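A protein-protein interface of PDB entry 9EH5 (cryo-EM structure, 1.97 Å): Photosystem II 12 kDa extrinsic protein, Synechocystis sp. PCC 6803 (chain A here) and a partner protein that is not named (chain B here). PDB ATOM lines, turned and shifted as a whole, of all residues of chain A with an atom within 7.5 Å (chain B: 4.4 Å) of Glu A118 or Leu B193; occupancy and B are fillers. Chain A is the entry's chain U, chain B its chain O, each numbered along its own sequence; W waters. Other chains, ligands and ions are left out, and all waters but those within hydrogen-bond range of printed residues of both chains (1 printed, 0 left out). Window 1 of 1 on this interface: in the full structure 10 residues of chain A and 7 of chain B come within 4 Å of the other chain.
O of Leu B193 sits at hydrogen-bond distance from ND2 of Asn A39 (3.2 Å).
Leu B193 touches just these residues of chain A: Asn A39 (3.2 Å), Ala A40 (3.9 Å), Val A41 (3.3 Å) and Glu A118 (3.9 Å).
Of the printed residues of chain A, Thr B217 touches Ile A117 and Glu A118.
Of the printed residues of chain B, Ala A40 touches Leu B193.
Of the printed residues of chain B, Asp A124 touches Tyr B194 (3.6 Å).
Leu A38 touches none of the printed residues of chain B.
The nearest residue of chain A that does not touch Leu B193 is Asp A42 (5.2 Å).
The nearest printed residue of chain B that does not touch Ile A117 is Ala B183 (6.1 Å).
Among the printed residues, pairs that only touch across the chains: Asn A39 with Gly B192 (3.98 Å), Asn A39 with Lys B215 (3.5 Å), Ala A40 with Leu B193 (3.9 Å), Val A41 with Leu B193 (3.3 Å), Val A41 with Tyr B194 (3.7 Å), Ile A117 with Thr B217 (3.1 Å), Glu A118 with Ala B183 (3.4 Å), Glu A118 with Leu B193 (3.9 Å), Glu A118 with Tyr B194 (3.5 Å), Glu A118 with Thr B217 (3.2 Å), Leu A119 with Tyr B194 (3.98 Å) and Asp A124 with Tyr B194 (3.6 Å).
Water W1 lies within hydrogen-bond range of the side-chain amide nitrogen of Asn A39, the backbone NH of Lys B215 and the backbone carbonyl oxygen of Gly B192.
The backbone carbonyl oxygen (O) of Ala B183 is in hydrogen-bond range of the backbone NH (N) of Tyr B194 (3.2 Å).
OD1 of Asn A39 lies within hydrogen-bond range of N of Asp A42.
The side-chain amide oxygen (OD1) of Asn A39 lies close to the backbone NH (N) of Val A41 (3.3 Å).
The backbone carbonyl oxygen of Ala B183 is in hydrogen-bond range of the backbone NH of Leu B193 (3.4 Å).
Hydrophobic or aromatic side chains of chain B within 4 Å of the printed part of chain A: Ala B183, Leu B193 and Tyr B194.
Of the 15 printed residues of chain A, 7 touch a printed residue of chain B.
Hydrophobic or aromatic side chains of chain A within 4 Å of the printed part of chain B: Val A41, Ile A117 and Leu A119.
Among the printed residues, 13 pairs touch across the chains.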
ATOM      1  N   LEU A  38      12.515  11.761 -22.228  1.00  0.00           N
ATOM      2  CA  LEU A  38      11.658  11.570 -21.070  1.00  0.00           C
ATOM      3  C   LEU A  38      12.108  10.365 -20.256  1.00  0.00           C
ATOM      4  O   LEU A  38      12.599   9.369 -20.796  1.00  0.00           O
ATOM      5  CB  LEU A  38      10.206  11.363 -21.501  1.00  0.00           C
ATOM      6  CG  LEU A  38       9.456  12.551 -22.097  1.00  0.00           C
ATOM      7  CD1 LEU A  38       8.068  12.117 -22.517  1.00  0.00           C
ATOM      8  CD2 LEU A  38       9.396  13.698 -21.111  1.00  0.00           C
ATOM      9  N   ASN A  39      11.912  10.448 -18.944  1.00  0.00           N
ATOM     10  CA  ASN A  39      12.037   9.256 -18.124  1.00  0.00           C
ATOM     11  C   ASN A  39      10.789   8.390 -18.296  1.00  0.00           C
ATOM     12  O   ASN A  39       9.837   8.751 -18.995  1.00  0.00           O
ATOM     13  CB  ASN A  39      12.327   9.625 -16.664  1.00  0.00           C
ATOM     14  CG  ASN A  39      11.225  10.469 -16.005  1.00  0.00           C
ATOM     15  OD1 ASN A  39      10.050  10.111 -15.986  1.00  0.00           O
ATOM     16  ND2 ASN A  39      11.631  11.590 -15.428  1.00  0.00           N
ATOM     17  N   ALA A  40      10.772   7.246 -17.614  1.00  0.00           N
ATOM     18  CA  ALA A  40       9.780   6.223 -17.924  1.00  0.00           C
ATOM     19  C   ALA A  40       8.392   6.582 -17.406  1.00  0.00           C
ATOM     20  O   ALA A  40       7.389   6.227 -18.034  1.00  0.00           O
ATOM     21  CB  ALA A  40      10.223   4.880 -17.365  1.00  0.00           C
ATOM     22  N   VAL A  41       8.298   7.275 -16.267  1.00  0.00           N
ATOM     23  CA  VAL A  41       6.967   7.614 -15.775  1.00  0.00           C
ATOM     24  C   VAL A  41       6.362   8.775 -16.554  1.00  0.00           C
ATOM     25  O   VAL A  41       5.133   8.874 -16.640  1.00  0.00           O
ATOM     26  CB  VAL A  41       6.963   7.896 -14.257  1.00  0.00           C
ATOM     27  CG1 VAL A  41       7.633   6.762 -13.504  1.00  0.00           C
ATOM     28  CG2 VAL A  41       7.621   9.213 -13.932  1.00  0.00           C
ATOM     29  N   ASP A  42       7.184   9.630 -17.173  1.00  0.00           N
ATOM     30  CA  ASP A  42       6.651  10.638 -18.085  1.00  0.00           C
ATOM     31  C   ASP A  42       6.068   9.986 -19.333  1.00  0.00           C
ATOM     32  O   ASP A  42       4.971  10.352 -19.780  1.00  0.00           O
ATOM     33  CB  ASP A  42       7.746  11.637 -18.462  1.00  0.00           C
ATOM     34  CG  ASP A  42       8.040  12.618 -17.352  1.00  0.00           C
ATOM     35  OD1 ASP A  42       7.104  12.939 -16.597  1.00  0.00           O
ATOM     36  OD2 ASP A  42       9.201  13.066 -17.231  1.00  0.00           O
ATOM     37  N   LYS A  44       4.922   7.101 -19.359  1.00  0.00           N
ATOM     38  CA  LYS A  44       3.676   6.413 -18.935  1.00  0.00           C
ATOM     39  C   LYS A  44       2.564   7.456 -18.871  1.00  0.00           C
ATOM     40  O   LYS A  44       1.425   7.117 -19.161  1.00  0.00           O
ATOM     41  CB  LYS A  44       3.844   5.700 -17.595  1.00  0.00           C
ATOM     42  CG  LYS A  44       2.934   4.501 -17.386  1.00  0.00           C
ATOM     43  CD  LYS A  44       3.594   3.383 -16.628  1.00  0.00           C
ATOM     44  CE  LYS A  44       3.109   2.021 -17.070  1.00  0.00           C
ATOM     45  NZ  LYS A  44       3.529   1.709 -18.455  1.00  0.00           N
ATOM     46  N   ASN A  57      -0.511  -0.257 -12.202  1.00  0.00           N
ATOM     47  CA  ASN A  57       0.486   0.768 -11.799  1.00  0.00           C
ATOM     48  C   ASN A  57      -0.103   1.864 -10.901  1.00  0.00           C
ATOM     49  O   ASN A  57       0.683   2.523 -10.224  1.00  0.00           O
ATOM     50  CB  ASN A  57       1.109   1.427 -13.026  1.00  0.00           C
ATOM     51  CG  ASN A  57       1.972   0.491 -13.839  1.00  0.00           C
ATOM     52  OD1 ASN A  57       3.138   0.287 -13.520  1.00  0.00           O
ATOM     53  ND2 ASN A  57       1.407  -0.072 -14.893  1.00  0.00           N
ATOM     54  N   PRO A 115       3.180  -3.333 -16.456  1.00  0.00           N
ATOM     55  CA  PRO A 115       3.625  -2.962 -15.106  1.00  0.00           C
ATOM     56  C   PRO A 115       5.026  -2.372 -15.157  1.00  0.00           C
ATOM     57  O   PRO A 115       5.962  -2.997 -15.656  1.00  0.00           O
ATOM     58  CB  PRO A 115       3.586  -4.288 -14.336  1.00  0.00           C
ATOM     59  CG  PRO A 115       3.576  -5.345 -15.365  1.00  0.00           C
ATOM     60  CD  PRO A 115       2.891  -4.772 -16.565  1.00  0.00           C
ATOM     61  N   SER A 116       5.150  -1.144 -14.675  1.00  0.00           N
ATOM     62  CA  SER A 116       6.428  -0.461 -14.584  1.00  0.00           C
ATOM     63  C   SER A 116       6.924  -0.568 -13.153  1.00  0.00           C
ATOM     64  O   SER A 116       6.217  -0.188 -12.215  1.00  0.00           O
ATOM     65  CB  SER A 116       6.292   1.005 -14.992  1.00  0.00           C
ATOM     66  OG  SER A 116       5.442   1.694 -14.097  1.00  0.00           O
ATOM     67  N   ILE A 117       8.135  -1.101 -12.991  1.00  0.00           N
ATOM     68  CA  ILE A 117       8.744  -1.251 -11.675  1.00  0.00           C
ATOM     69  C   ILE A 117       9.025   0.074 -10.971  1.00  0.00           C
ATOM     70  O   ILE A 117       9.127   0.102  -9.743  1.00  0.00           O
ATOM     71  CB  ILE A 117       9.939  -2.228 -11.873  1.00  0.00           C
ATOM     72  CG1 ILE A 117      11.073  -1.743 -12.806  1.00  0.00           C
ATOM     73  CG2 ILE A 117       9.500  -3.530 -12.472  1.00  0.00           C
ATOM     74  CD1 ILE A 117      11.883  -0.653 -12.400  1.00  0.00           C
ATOM     75  N   GLU A 118       9.138   1.168 -11.725  1.00  0.00           N
ATOM     76  CA  GLU A 118       9.375   2.494 -11.168  1.00  0.00           C
ATOM     77  C   GLU A 118       8.211   2.987 -10.307  1.00  0.00           C
ATOM     78  O   GLU A 118       8.404   3.863  -9.455  1.00  0.00           O
ATOM     79  CB  GLU A 118       9.665   3.450 -12.332  1.00  0.00           C
ATOM     80  CG  GLU A 118      10.874   2.981 -13.140  1.00  0.00           C
ATOM     81  CD  GLU A 118      10.559   2.516 -14.557  1.00  0.00           C
ATOM     82  OE1 GLU A 118      11.458   2.630 -15.410  1.00  0.00           O
ATOM     83  OE2 GLU A 118       9.432   2.051 -14.827  1.00  0.00           O
ATOM     84  N   LEU A 119       7.014   2.440 -10.507  1.00  0.00           N
ATOM     85  CA  LEU A 119       5.864   2.736  -9.671  1.00  0.00           C
ATOM     86  C   LEU A 119       5.485   1.594  -8.738  1.00  0.00           C
ATOM     87  O   LEU A 119       4.659   1.801  -7.844  1.00  0.00           O
ATOM     88  CB  LEU A 119       4.662   3.095 -10.557  1.00  0.00           C
ATOM     89  CG  LEU A 119       4.981   4.169 -11.597  1.00  0.00           C
ATOM     90  CD1 LEU A 119       3.878   4.245 -12.643  1.00  0.00           C
ATOM     91  CD2 LEU A 119       5.198   5.527 -10.939  1.00  0.00           C
ATOM     92  N   THR A 120       6.057   0.396  -8.913  1.00  0.00           N
ATOM     93  CA  THR A 120       5.620  -0.759  -8.139  1.00  0.00           C
ATOM     94  C   THR A 120       6.665  -1.320  -7.183  1.00  0.00           C
ATOM     95  O   THR A 120       6.291  -2.050  -6.260  1.00  0.00           O
ATOM     96  CB  THR A 120       5.168  -1.899  -9.068  1.00  0.00           C
ATOM     97  OG1 THR A 120       6.265  -2.335  -9.876  1.00  0.00           O
ATOM     98  CG2 THR A 120       4.048  -1.437  -9.978  1.00  0.00           C
ATOM     99  N   SER A 121       7.946  -1.023  -7.381  1.00  0.00           N
ATOM    100  CA  SER A 121       8.985  -1.567  -6.518  1.00  0.00           C
ATOM    101  C   SER A 121       8.980  -0.874  -5.162  1.00  0.00           C
ATOM    102  O   SER A 121       8.918   0.350  -5.068  1.00  0.00           O
ATOM    103  CB  SER A 121      10.356  -1.403  -7.169  1.00  0.00           C
ATOM    104  OG  SER A 121      10.980  -0.211  -6.727  1.00  0.00           O
ATOM    105  N   ASP A 124       5.377   1.248  -3.703  1.00  0.00           N
ATOM    106  CA  ASP A 124       4.936   2.615  -3.953  1.00  0.00           C
ATOM    107  C   ASP A 124       3.462   2.682  -4.309  1.00  0.00           C
ATOM    108  O   ASP A 124       2.875   3.762  -4.216  1.00  0.00           O
ATOM    109  CB  ASP A 124       5.717   3.302  -5.078  1.00  0.00           C
ATOM    110  CG  ASP A 124       7.204   3.091  -4.987  1.00  0.00           C
ATOM    111  OD1 ASP A 124       7.789   3.393  -3.927  1.00  0.00           O
ATOM    112  OD2 ASP A 124       7.795   2.715  -6.020  1.00  0.00           O
ATOM    113  N   ALA B 183      12.615   5.388  -7.186  1.00  0.00           N
ATOM    114  CA  ALA B 183      12.175   6.407  -8.124  1.00  0.00           C
ATOM    115  C   ALA B 183      11.684   7.680  -7.438  1.00  0.00           C
ATOM    116  O   ALA B 183      11.461   8.683  -8.125  1.00  0.00           O
ATOM    117  CB  ALA B 183      11.092   5.827  -9.033  1.00  0.00           C
ATOM    118  N   GLY B 192      14.719  13.621 -10.028  1.00  0.00           N
ATOM    119  CA  GLY B 192      14.448  12.217  -9.786  1.00  0.00           C
ATOM    120  C   GLY B 192      13.549  11.646 -10.862  1.00  0.00           C
ATOM    121  O   GLY B 192      13.422  12.240 -11.935  1.00  0.00           O
ATOM    122  N   LEU B 193      12.905  10.509 -10.597  1.00  0.00           N
ATOM    123  CA  LEU B 193      12.163   9.818 -11.659  1.00  0.00           C
ATOM    124  C   LEU B 193      10.690  10.220 -11.673  1.00  0.00           C
ATOM    125  O   LEU B 193      10.228  10.847 -12.629  1.00  0.00           O
ATOM    126  CB  LEU B 193      12.337   8.306 -11.520  1.00  0.00           C
ATOM    127  CG  LEU B 193      12.563   7.534 -12.828  1.00  0.00           C
ATOM    128  CD1 LEU B 193      13.051   6.144 -12.505  1.00  0.00           C
ATOM    129  CD2 LEU B 193      11.324   7.468 -13.713  1.00  0.00           C
ATOM    130  N   TYR B 194       9.941   9.890 -10.617  1.00  0.00           N
ATOM    131  CA  TYR B 194       8.546  10.318 -10.558  1.00  0.00           C
ATOM    132  C   TYR B 194       8.351  11.587  -9.743  1.00  0.00           C
ATOM    133  O   TYR B 194       7.210  12.005  -9.533  1.00  0.00           O
ATOM    134  CB  TYR B 194       7.617   9.182 -10.062  1.00  0.00           C
ATOM    135  CG  TYR B 194       7.787   8.571  -8.667  1.00  0.00           C
ATOM    136  CD1 TYR B 194       7.884   7.195  -8.522  1.00  0.00           C
ATOM    137  CD2 TYR B 194       7.733   9.337  -7.500  1.00  0.00           C
ATOM    138  CE1 TYR B 194       8.016   6.611  -7.271  1.00  0.00           C
ATOM    139  CE2 TYR B 194       7.852   8.771  -6.264  1.00  0.00           C
ATOM    140  CZ  TYR B 194       7.996   7.410  -6.147  1.00  0.00           C
ATOM    141  OH  TYR B 194       8.115   6.855  -4.896  1.00  0.00           O
ATOM    142  N   THR B 195       9.429  12.181  -9.255  1.00  0.00           N
ATOM    143  CA  THR B 195       9.373  13.466  -8.585  1.00  0.00           C
ATOM    144  C   THR B 195      10.623  14.243  -8.961  1.00  0.00           C
ATOM    145  O   THR B 195      11.614  13.663  -9.395  1.00  0.00           O
ATOM    146  CB  THR B 195       9.255  13.329  -7.062  1.00  0.00           C
ATOM    147  OG1 THR B 195       9.280  14.629  -6.462  1.00  0.00           O
ATOM    148  CG2 THR B 195      10.397  12.494  -6.504  1.00  0.00           C
ATOM    149  N   LYS B 215      16.626  10.245 -15.238  1.00  0.00           N
ATOM    150  CA  LYS B 215      16.880   9.165 -14.300  1.00  0.00           C
ATOM    151  C   LYS B 215      16.141   7.906 -14.734  1.00  0.00           C
ATOM    152  O   LYS B 215      15.099   7.967 -15.390  1.00  0.00           O
ATOM    153  CB  LYS B 215      16.458   9.561 -12.884  1.00  0.00           C
ATOM    154  CG  LYS B 215      16.907  10.953 -12.462  1.00  0.00           C
ATOM    155  CD  LYS B 215      18.420  11.044 -12.324  1.00  0.00           C
ATOM    156  CE  LYS B 215      18.828  12.189 -11.407  1.00  0.00           C
ATOM    157  NZ  LYS B 215      20.272  12.516 -11.546  1.00  0.00           N
ATOM    158  N   GLU B 216      16.704   6.758 -14.373  1.00  0.00           N
ATOM    159  CA  GLU B 216      16.089   5.469 -14.650  1.00  0.00           C
ATOM    160  C   GLU B 216      16.483   4.497 -13.548  1.00  0.00           C
ATOM    161  O   GLU B 216      17.544   4.634 -12.939  1.00  0.00           O
ATOM    162  CB  GLU B 216      16.516   4.912 -16.014  1.00  0.00           C
ATOM    163  CG  GLU B 216      18.018   4.809 -16.202  1.00  0.00           C
ATOM    164  CD  GLU B 216      18.453   5.201 -17.598  1.00  0.00           C
ATOM    165  OE1 GLU B 216      17.574   5.507 -18.425  1.00  0.00           O
ATOM    166  OE2 GLU B 216      19.671   5.212 -17.866  1.00  0.00           O
ATOM    167  N   THR B 217      15.622   3.521 -13.282  1.00  0.00           N
ATOM    168  CA  THR B 217      15.876   2.514 -12.251  1.00  0.00           C
ATOM    169  C   THR B 217      15.679   1.115 -12.815  1.00  0.00           C
ATOM    170  O   THR B 217      14.735   0.445 -12.424  1.00  0.00           O
ATOM    171  CB  THR B 217      14.938   2.694 -11.052  1.00  0.00           C
ATOM    172  OG1 THR B 217      13.572   2.584 -11.472  1.00  0.00           O
ATOM    173  CG2 THR B 217      15.148   4.002 -10.332  1.00  0.00           C
HETATM  174  O   HOH W   1      14.315  12.056 -14.911  1.00  0.00           O
